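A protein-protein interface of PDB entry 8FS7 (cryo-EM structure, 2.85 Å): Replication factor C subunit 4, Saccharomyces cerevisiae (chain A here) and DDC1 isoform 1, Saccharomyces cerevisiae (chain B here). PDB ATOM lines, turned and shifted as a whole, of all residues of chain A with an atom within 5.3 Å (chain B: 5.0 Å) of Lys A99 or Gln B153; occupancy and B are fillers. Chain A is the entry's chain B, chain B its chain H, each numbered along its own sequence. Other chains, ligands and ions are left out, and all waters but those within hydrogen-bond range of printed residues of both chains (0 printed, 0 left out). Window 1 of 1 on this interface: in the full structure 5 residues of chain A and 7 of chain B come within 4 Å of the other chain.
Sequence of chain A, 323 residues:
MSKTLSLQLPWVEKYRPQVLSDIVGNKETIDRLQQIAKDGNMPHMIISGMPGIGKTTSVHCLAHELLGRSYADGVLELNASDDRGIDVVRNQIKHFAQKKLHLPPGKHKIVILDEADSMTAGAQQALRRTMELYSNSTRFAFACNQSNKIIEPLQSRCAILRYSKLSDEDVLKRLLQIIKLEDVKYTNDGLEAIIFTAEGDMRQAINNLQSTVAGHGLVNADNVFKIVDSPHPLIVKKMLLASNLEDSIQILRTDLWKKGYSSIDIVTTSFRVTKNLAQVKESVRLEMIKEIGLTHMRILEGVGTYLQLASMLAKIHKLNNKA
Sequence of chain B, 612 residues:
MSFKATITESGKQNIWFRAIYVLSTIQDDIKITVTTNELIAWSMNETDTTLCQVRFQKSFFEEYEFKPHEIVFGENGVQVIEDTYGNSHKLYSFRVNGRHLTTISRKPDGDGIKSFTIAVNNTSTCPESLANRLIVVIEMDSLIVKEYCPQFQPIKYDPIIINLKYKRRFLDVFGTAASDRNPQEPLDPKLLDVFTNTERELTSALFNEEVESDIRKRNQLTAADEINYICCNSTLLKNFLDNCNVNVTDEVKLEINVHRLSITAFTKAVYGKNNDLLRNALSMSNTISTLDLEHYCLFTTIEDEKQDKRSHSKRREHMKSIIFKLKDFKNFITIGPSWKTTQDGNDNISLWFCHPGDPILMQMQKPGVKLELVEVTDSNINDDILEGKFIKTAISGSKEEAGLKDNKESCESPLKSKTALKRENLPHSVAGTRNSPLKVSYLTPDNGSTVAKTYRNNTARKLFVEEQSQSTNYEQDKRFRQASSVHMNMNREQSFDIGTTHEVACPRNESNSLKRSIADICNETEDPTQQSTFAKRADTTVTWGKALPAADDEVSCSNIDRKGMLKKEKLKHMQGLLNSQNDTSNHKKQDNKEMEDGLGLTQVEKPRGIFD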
ATOM      1  N   ASP A  73     -25.355 -15.022   5.237  1.00  0.00           N
ATOM      2  CA  ASP A  73     -25.471 -16.354   4.653  1.00  0.00           C
ATOM      3  C   ASP A  73     -24.850 -17.421   5.549  1.00  0.00           C
ATOM      4  O   ASP A  73     -24.405 -18.465   5.067  1.00  0.00           O
ATOM      5  CB  ASP A  73     -24.839 -16.387   3.262  1.00  0.00           C
ATOM      6  CG  ASP A  73     -23.388 -15.952   3.271  1.00  0.00           C
ATOM      7  OD1 ASP A  73     -23.105 -14.829   3.737  1.00  0.00           O
ATOM      8  OD2 ASP A  73     -22.529 -16.735   2.811  1.00  0.00           O
ATOM      9  N   GLY A  74     -24.813 -17.174   6.856  1.00  0.00           N
ATOM     10  CA  GLY A  74     -24.284 -18.152   7.786  1.00  0.00           C
ATOM     11  C   GLY A  74     -25.275 -18.574   8.849  1.00  0.00           C
ATOM     12  O   GLY A  74     -25.013 -19.506   9.613  1.00  0.00           O
ATOM     13  N   LYS A  94     -31.257 -29.579   5.558  1.00  0.00           N
ATOM     14  CA  LYS A  94     -30.230 -30.403   4.932  1.00  0.00           C
ATOM     15  C   LYS A  94     -29.394 -29.588   3.952  1.00  0.00           C
ATOM     16  O   LYS A  94     -28.171 -29.751   3.881  1.00  0.00           O
ATOM     17  CB  LYS A  94     -30.871 -31.602   4.233  1.00  0.00           C
ATOM     18  CG  LYS A  94     -29.867 -32.576   3.635  1.00  0.00           C
ATOM     19  CD  LYS A  94     -30.463 -33.964   3.469  1.00  0.00           C
ATOM     20  CE  LYS A  94     -31.786 -33.916   2.722  1.00  0.00           C
ATOM     21  NZ  LYS A  94     -31.637 -33.309   1.372  1.00  0.00           N
ATOM     22  N   HIS A  95     -30.036 -28.700   3.187  1.00  0.00           N
ATOM     23  CA  HIS A  95     -29.288 -27.889   2.231  1.00  0.00           C
ATOM     24  C   HIS A  95     -28.391 -26.879   2.938  1.00  0.00           C
ATOM     25  O   HIS A  95     -27.266 -26.622   2.494  1.00  0.00           O
ATOM     26  CB  HIS A  95     -30.250 -27.184   1.275  1.00  0.00           C
ATOM     27  CG  HIS A  95     -31.027 -28.122   0.405  1.00  0.00           C
ATOM     28  ND1 HIS A  95     -30.662 -29.439   0.219  1.00  0.00           N
ATOM     29  CD2 HIS A  95     -32.150 -27.936  -0.329  1.00  0.00           C
ATOM     30  CE1 HIS A  95     -31.527 -30.023  -0.591  1.00  0.00           C
ATOM     31  NE2 HIS A  95     -32.440 -29.133  -0.938  1.00  0.00           N
ATOM     32  N   PHE A  96     -28.872 -26.293   4.036  1.00  0.00           N
ATOM     33  CA  PHE A  96     -28.065 -25.320   4.768  1.00  0.00           C
ATOM     34  C   PHE A  96     -26.915 -25.996   5.506  1.00  0.00           C
ATOM     35  O   PHE A  96     -25.804 -25.456   5.560  1.00  0.00           O
ATOM     36  CB  PHE A  96     -28.948 -24.539   5.741  1.00  0.00           C
ATOM     37  CG  PHE A  96     -28.213 -23.488   6.521  1.00  0.00           C
ATOM     38  CD1 PHE A  96     -27.903 -22.268   5.942  1.00  0.00           C
ATOM     39  CD2 PHE A  96     -27.839 -23.713   7.835  1.00  0.00           C
ATOM     40  CE1 PHE A  96     -27.229 -21.297   6.656  1.00  0.00           C
ATOM     41  CE2 PHE A  96     -27.165 -22.747   8.555  1.00  0.00           C
ATOM     42  CZ  PHE A  96     -26.860 -21.537   7.964  1.00  0.00           C
ATOM     43  N   ALA A  97     -27.164 -27.173   6.085  1.00  0.00           N
ATOM     44  CA  ALA A  97     -26.112 -27.890   6.797  1.00  0.00           C
ATOM     45  C   ALA A  97     -25.046 -28.405   5.840  1.00  0.00           C
ATOM     46  O   ALA A  97     -23.851 -28.376   6.159  1.00  0.00           O
ATOM     47  CB  ALA A  97     -26.717 -29.044   7.597  1.00  0.00           C
ATOM     48  N   GLN A  98     -25.456 -28.882   4.663  1.00  0.00           N
ATOM     49  CA  GLN A  98     -24.499 -29.393   3.689  1.00  0.00           C
ATOM     50  C   GLN A  98     -23.658 -28.290   3.064  1.00  0.00           C
ATOM     51  O   GLN A  98     -22.586 -28.583   2.525  1.00  0.00           O
ATOM     52  CB  GLN A  98     -25.223 -30.169   2.589  1.00  0.00           C
ATOM     53  CG  GLN A  98     -25.637 -31.575   2.982  1.00  0.00           C
ATOM     54  CD  GLN A  98     -26.444 -32.266   1.901  1.00  0.00           C
ATOM     55  OE1 GLN A  98     -27.124 -31.616   1.107  1.00  0.00           O
ATOM     56  NE2 GLN A  98     -26.374 -33.592   1.866  1.00  0.00           N
ATOM     57  N   LYS A  99     -24.116 -27.040   3.118  1.00  0.00           N
ATOM     58  CA  LYS A  99     -23.406 -25.945   2.470  1.00  0.00           C
ATOM     59  C   LYS A  99     -22.012 -25.776   3.064  1.00  0.00           C
ATOM     60  O   LYS A  99     -21.845 -25.715   4.286  1.00  0.00           O
ATOM     61  CB  LYS A  99     -24.203 -24.648   2.610  1.00  0.00           C
ATOM     62  CG  LYS A  99     -23.469 -23.410   2.124  1.00  0.00           C
ATOM     63  CD  LYS A  99     -24.352 -22.175   2.205  1.00  0.00           C
ATOM     64  CE  LYS A  99     -24.855 -21.944   3.621  1.00  0.00           C
ATOM     65  NZ  LYS A  99     -25.760 -20.765   3.699  1.00  0.00           N
ATOM     66  N   LYS A 100     -21.011 -25.700   2.189  1.00  0.00           N
ATOM     67  CA  LYS A 100     -19.614 -25.568   2.601  1.00  0.00           C
ATOM     68  C   LYS A 100     -19.247 -24.091   2.565  1.00  0.00           C
ATOM     69  O   LYS A 100     -18.750 -23.572   1.564  1.00  0.00           O
ATOM     70  CB  LYS A 100     -18.706 -26.397   1.704  1.00  0.00           C
ATOM     71  CG  LYS A 100     -18.268 -27.720   2.316  1.00  0.00           C
ATOM     72  CD  LYS A 100     -16.925 -28.176   1.765  1.00  0.00           C
ATOM     73  CE  LYS A 100     -15.885 -27.066   1.831  1.00  0.00           C
ATOM     74  NZ  LYS A 100     -15.723 -26.530   3.211  1.00  0.00           N
ATOM     75  N   LEU A 101     -19.493 -23.404   3.676  1.00  0.00           N
ATOM     76  CA  LEU A 101     -19.184 -21.988   3.813  1.00  0.00           C
ATOM     77  C   LEU A 101     -17.887 -21.840   4.597  1.00  0.00           C
ATOM     78  O   LEU A 101     -17.778 -22.341   5.722  1.00  0.00           O
ATOM     79  CB  LEU A 101     -20.326 -21.247   4.508  1.00  0.00           C
ATOM     80  CG  LEU A 101     -20.008 -19.855   5.055  1.00  0.00           C
ATOM     81  CD1 LEU A 101     -20.274 -18.793   4.004  1.00  0.00           C
ATOM     82  CD2 LEU A 101     -20.820 -19.581   6.311  1.00  0.00           C
ATOM     83  N   LYS A 109     -21.602 -22.495  11.411  1.00  0.00           N
ATOM     84  CA  LYS A 109     -22.923 -22.009  11.043  1.00  0.00           C
ATOM     85  C   LYS A 109     -23.905 -22.229  12.188  1.00  0.00           C
ATOM     86  O   LYS A 109     -23.789 -23.183  12.961  1.00  0.00           O
ATOM     87  CB  LYS A 109     -23.423 -22.710   9.780  1.00  0.00           C
ATOM     88  CG  LYS A 109     -22.655 -22.347   8.519  1.00  0.00           C
ATOM     89  CD  LYS A 109     -23.069 -23.224   7.348  1.00  0.00           C
ATOM     90  CE  LYS A 109     -22.856 -24.697   7.656  1.00  0.00           C
ATOM     91  NZ  LYS A 109     -23.224 -25.565   6.504  1.00  0.00           N
ATOM     92  N   ASP B  29     -28.176 -37.122  -4.207  1.00  0.00           N
ATOM     93  CA  ASP B  29     -27.033 -36.285  -4.544  1.00  0.00           C
ATOM     94  C   ASP B  29     -26.237 -36.944  -5.659  1.00  0.00           C
ATOM     95  O   ASP B  29     -25.952 -38.144  -5.598  1.00  0.00           O
ATOM     96  CB  ASP B  29     -26.141 -36.045  -3.320  1.00  0.00           C
ATOM     97  CG  ASP B  29     -26.407 -34.707  -2.659  1.00  0.00           C
ATOM     98  OD1 ASP B  29     -27.582 -34.284  -2.625  1.00  0.00           O
ATOM     99  OD2 ASP B  29     -25.445 -34.077  -2.175  1.00  0.00           O
ATOM    100  N   SER B  93     -13.368 -33.750  -7.903  1.00  0.00           N
ATOM    101  CA  SER B  93     -14.677 -34.343  -7.671  1.00  0.00           C
ATOM    102  C   SER B  93     -15.491 -33.445  -6.753  1.00  0.00           C
ATOM    103  O   SER B  93     -14.937 -32.769  -5.880  1.00  0.00           O
ATOM    104  CB  SER B  93     -14.553 -35.741  -7.054  1.00  0.00           C
ATOM    105  OG  SER B  93     -15.824 -36.351  -6.918  1.00  0.00           O
ATOM    106  N   PHE B  94     -16.808 -33.441  -6.953  1.00  0.00           N
ATOM    107  CA  PHE B  94     -17.698 -32.641  -6.127  1.00  0.00           C
ATOM    108  C   PHE B  94     -19.074 -33.291  -6.092  1.00  0.00           C
ATOM    109  O   PHE B  94     -19.423 -34.106  -6.951  1.00  0.00           O
ATOM    110  CB  PHE B  94     -17.789 -31.194  -6.628  1.00  0.00           C
ATOM    111  CG  PHE B  94     -18.263 -31.063  -8.050  1.00  0.00           C
ATOM    112  CD1 PHE B  94     -17.366 -31.129  -9.104  1.00  0.00           C
ATOM    113  CD2 PHE B  94     -19.604 -30.853  -8.331  1.00  0.00           C
ATOM    114  CE1 PHE B  94     -17.798 -31.002 -10.411  1.00  0.00           C
ATOM    115  CE2 PHE B  94     -20.042 -30.726  -9.636  1.00  0.00           C
ATOM    116  CZ  PHE B  94     -19.138 -30.800 -10.676  1.00  0.00           C
ATOM    117  N   ARG B  95     -19.852 -32.917  -5.080  1.00  0.00           N
ATOM    118  CA  ARG B  95     -21.180 -33.467  -4.845  1.00  0.00           C
ATOM    119  C   ARG B  95     -22.224 -32.378  -5.055  1.00  0.00           C
ATOM    120  O   ARG B  95     -22.129 -31.301  -4.459  1.00  0.00           O
ATOM    121  CB  ARG B  95     -21.288 -34.035  -3.428  1.00  0.00           C
ATOM    122  CG  ARG B  95     -21.893 -35.426  -3.350  1.00  0.00           C
ATOM    123  CD  ARG B  95     -22.625 -35.684  -2.031  1.00  0.00           C
ATOM    124  NE  ARG B  95     -21.903 -35.206  -0.856  1.00  0.00           N
ATOM    125  CZ  ARG B  95     -22.172 -34.076  -0.215  1.00  0.00           C
ATOM    126  NH1 ARG B  95     -23.147 -33.273  -0.608  1.00  0.00           N
ATOM    127  NH2 ARG B  95     -21.443 -33.743   0.847  1.00  0.00           N
ATOM    128  N   ASN B 132     -17.533 -22.329  -4.035  1.00  0.00           N
ATOM    129  CA  ASN B 132     -18.338 -23.518  -3.746  1.00  0.00           C
ATOM    130  C   ASN B 132     -19.715 -23.440  -4.401  1.00  0.00           C
ATOM    131  O   ASN B 132     -20.699 -23.963  -3.873  1.00  0.00           O
ATOM    132  CB  ASN B 132     -18.470 -23.761  -2.238  1.00  0.00           C
ATOM    133  CG  ASN B 132     -17.280 -24.501  -1.660  1.00  0.00           C
ATOM    134  OD1 ASN B 132     -17.131 -25.708  -1.854  1.00  0.00           O
ATOM    135  ND2 ASN B 132     -16.426 -23.782  -0.942  1.00  0.00           N
ATOM    136  N   GLN B 151     -25.251 -25.031  -5.193  1.00  0.00           N
ATOM    137  CA  GLN B 151     -24.189 -25.321  -4.241  1.00  0.00           C
ATOM    138  C   GLN B 151     -23.619 -26.710  -4.492  1.00  0.00           C
ATOM    139  O   GLN B 151     -24.357 -27.654  -4.790  1.00  0.00           O
ATOM    140  CB  GLN B 151     -24.716 -25.226  -2.810  1.00  0.00           C
ATOM    141  CG  GLN B 151     -25.524 -23.972  -2.523  1.00  0.00           C
ATOM    142  CD  GLN B 151     -24.733 -22.931  -1.755  1.00  0.00           C
ATOM    143  OE1 GLN B 151     -23.536 -23.093  -1.520  1.00  0.00           O
ATOM    144  NE2 GLN B 151     -25.402 -21.854  -1.359  1.00  0.00           N
ATOM    145  N   PHE B 152     -22.299 -26.834  -4.376  1.00  0.00           N
ATOM    146  CA  PHE B 152     -21.638 -28.126  -4.476  1.00  0.00           C
ATOM    147  C   PHE B 152     -20.678 -28.302  -3.307  1.00  0.00           C
ATOM    148  O   PHE B 152     -20.286 -27.338  -2.643  1.00  0.00           O
ATOM    149  CB  PHE B 152     -20.903 -28.304  -5.823  1.00  0.00           C
ATOM    150  CG  PHE B 152     -19.643 -27.484  -5.967  1.00  0.00           C
ATOM    151  CD1 PHE B 152     -18.422 -27.966  -5.515  1.00  0.00           C
ATOM    152  CD2 PHE B 152     -19.675 -26.251  -6.591  1.00  0.00           C
ATOM    153  CE1 PHE B 152     -17.269 -27.222  -5.657  1.00  0.00           C
ATOM    154  CE2 PHE B 152     -18.521 -25.505  -6.741  1.00  0.00           C
ATOM    155  CZ  PHE B 152     -17.318 -25.990  -6.270  1.00  0.00           C
ATOM    156  N   GLN B 153     -20.303 -29.556  -3.064  1.00  0.00           N
ATOM    157  CA  GLN B 153     -19.407 -29.912  -1.968  1.00  0.00           C
ATOM    158  C   GLN B 153     -18.303 -30.806  -2.516  1.00  0.00           C
ATOM    159  O   GLN B 153     -18.602 -31.895  -3.050  1.00  0.00           O
ATOM    160  CB  GLN B 153     -20.172 -30.615  -0.846  1.00  0.00           C
ATOM    161  CG  GLN B 153     -20.979 -29.677   0.025  1.00  0.00           C
ATOM    162  CD  GLN B 153     -22.438 -29.616  -0.384  1.00  0.00           C
ATOM    163  OE1 GLN B 153     -23.087 -30.646  -0.572  1.00  0.00           O
ATOM    164  NE2 GLN B 153     -22.963 -28.405  -0.524  1.00  0.00           N
ATOM    165  N   PRO B 154     -17.037 -30.402  -2.425  1.00  0.00           N
ATOM    166  CA  PRO B 154     -15.953 -31.264  -2.911  1.00  0.00           C
ATOM    167  C   PRO B 154     -15.854 -32.547  -2.098  1.00  0.00           C
ATOM    168  O   PRO B 154     -15.981 -32.540  -0.872  1.00  0.00           O
ATOM    169  CB  PRO B 154     -14.703 -30.391  -2.743  1.00  0.00           C
ATOM    170  CG  PRO B 154     -15.080 -29.373  -1.717  1.00  0.00           C
ATOM    171  CD  PRO B 154     -16.541 -29.115  -1.911  1.00  0.00           C
ATOM    172  N   ILE B 155     -15.625 -33.657  -2.799  1.00  0.00           N
ATOM    173  CA  ILE B 155     -15.504 -34.980  -2.202  1.00  0.00           C
ATOM    174  C   ILE B 155     -14.308 -35.688  -2.830  1.00  0.00           C
ATOM    175  O   ILE B 155     -13.573 -35.115  -3.638  1.00  0.00           O
ATOM    176  CB  ILE B 155     -16.783 -35.827  -2.380  1.00  0.00           C
ATOM    177  CG1 ILE B 155     -17.039 -36.097  -3.863  1.00  0.00           C
ATOM    178  CG2 ILE B 155     -17.984 -35.157  -1.724  1.00  0.00           C
ATOM    179  CD1 ILE B 155     -17.622 -37.461  -4.137  1.00  0.00           C
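Of the 10 printed residues of chain B, 4 touch a printed residue of chain A.
Hydrophobic or aromatic side chains of chain B within 4 Å of the printed part of chain A: Pro B154.
Along chain B the printed residues that touch a printed residue of chain A span positions 132 to 154.
Among the printed residues, 5 pairs touch across the chains.
Among the printed residues, no Asp or Glu carboxylate lies within 4 Å of a Lys or Arg side-chain nitrogen of the other chain.
Among the printed residues, merely in contact across the chains: Lys A99 with Gln B151 (3.7 Å), Lys A100 with Pro B154 (3.8 Å) and Lys A99 with Gln B153 (3.9 Å).
The backbone carbonyl oxygen of Gln A98 lies within hydrogen-bond range of the side-chain amide nitrogen of Gln B153 (3.1 Å).
The backbone carbonyl oxygen (O) of Lys A100 is in hydrogen-bond range of the side-chain amide nitrogen (ND2) of Asn B132 (3.4 Å).
Printed residues of chain B within 4 Å of Lys A99: Gln B151 and Gln B153.
Of chain A, only Gln A98 (3.1 Å) and Lys A99 (3.9 Å) come within 4 Å of Gln B153.
Printed residues of chain A within 4 Å of Asn B132: Lys A100 (3.4 Å).
Of the printed residues of chain A, Pro B154 touches Lys A100.
The nearest residue of chain A that does not touch Gln B153 is Lys A100 (4.1 Å).
The backbone carbonyl oxygen (O) of Lys A99 is in hydrogen-bond range of the side-chain amino group (NZ) of Lys A109.
The backbone NH (N) of Phe B152 sits at hydrogen-bond distance from the backbone carbonyl oxygen (O) of Asn B132 (3.3 Å).
O of Asp A73 sits at hydrogen-bond distance from NZ of Lys A99, 3.0 Å away.
The backbone NH of Arg B95 sits at hydrogen-bond distance from the backbone carbonyl oxygen of Gln B153 (2.6 Å).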
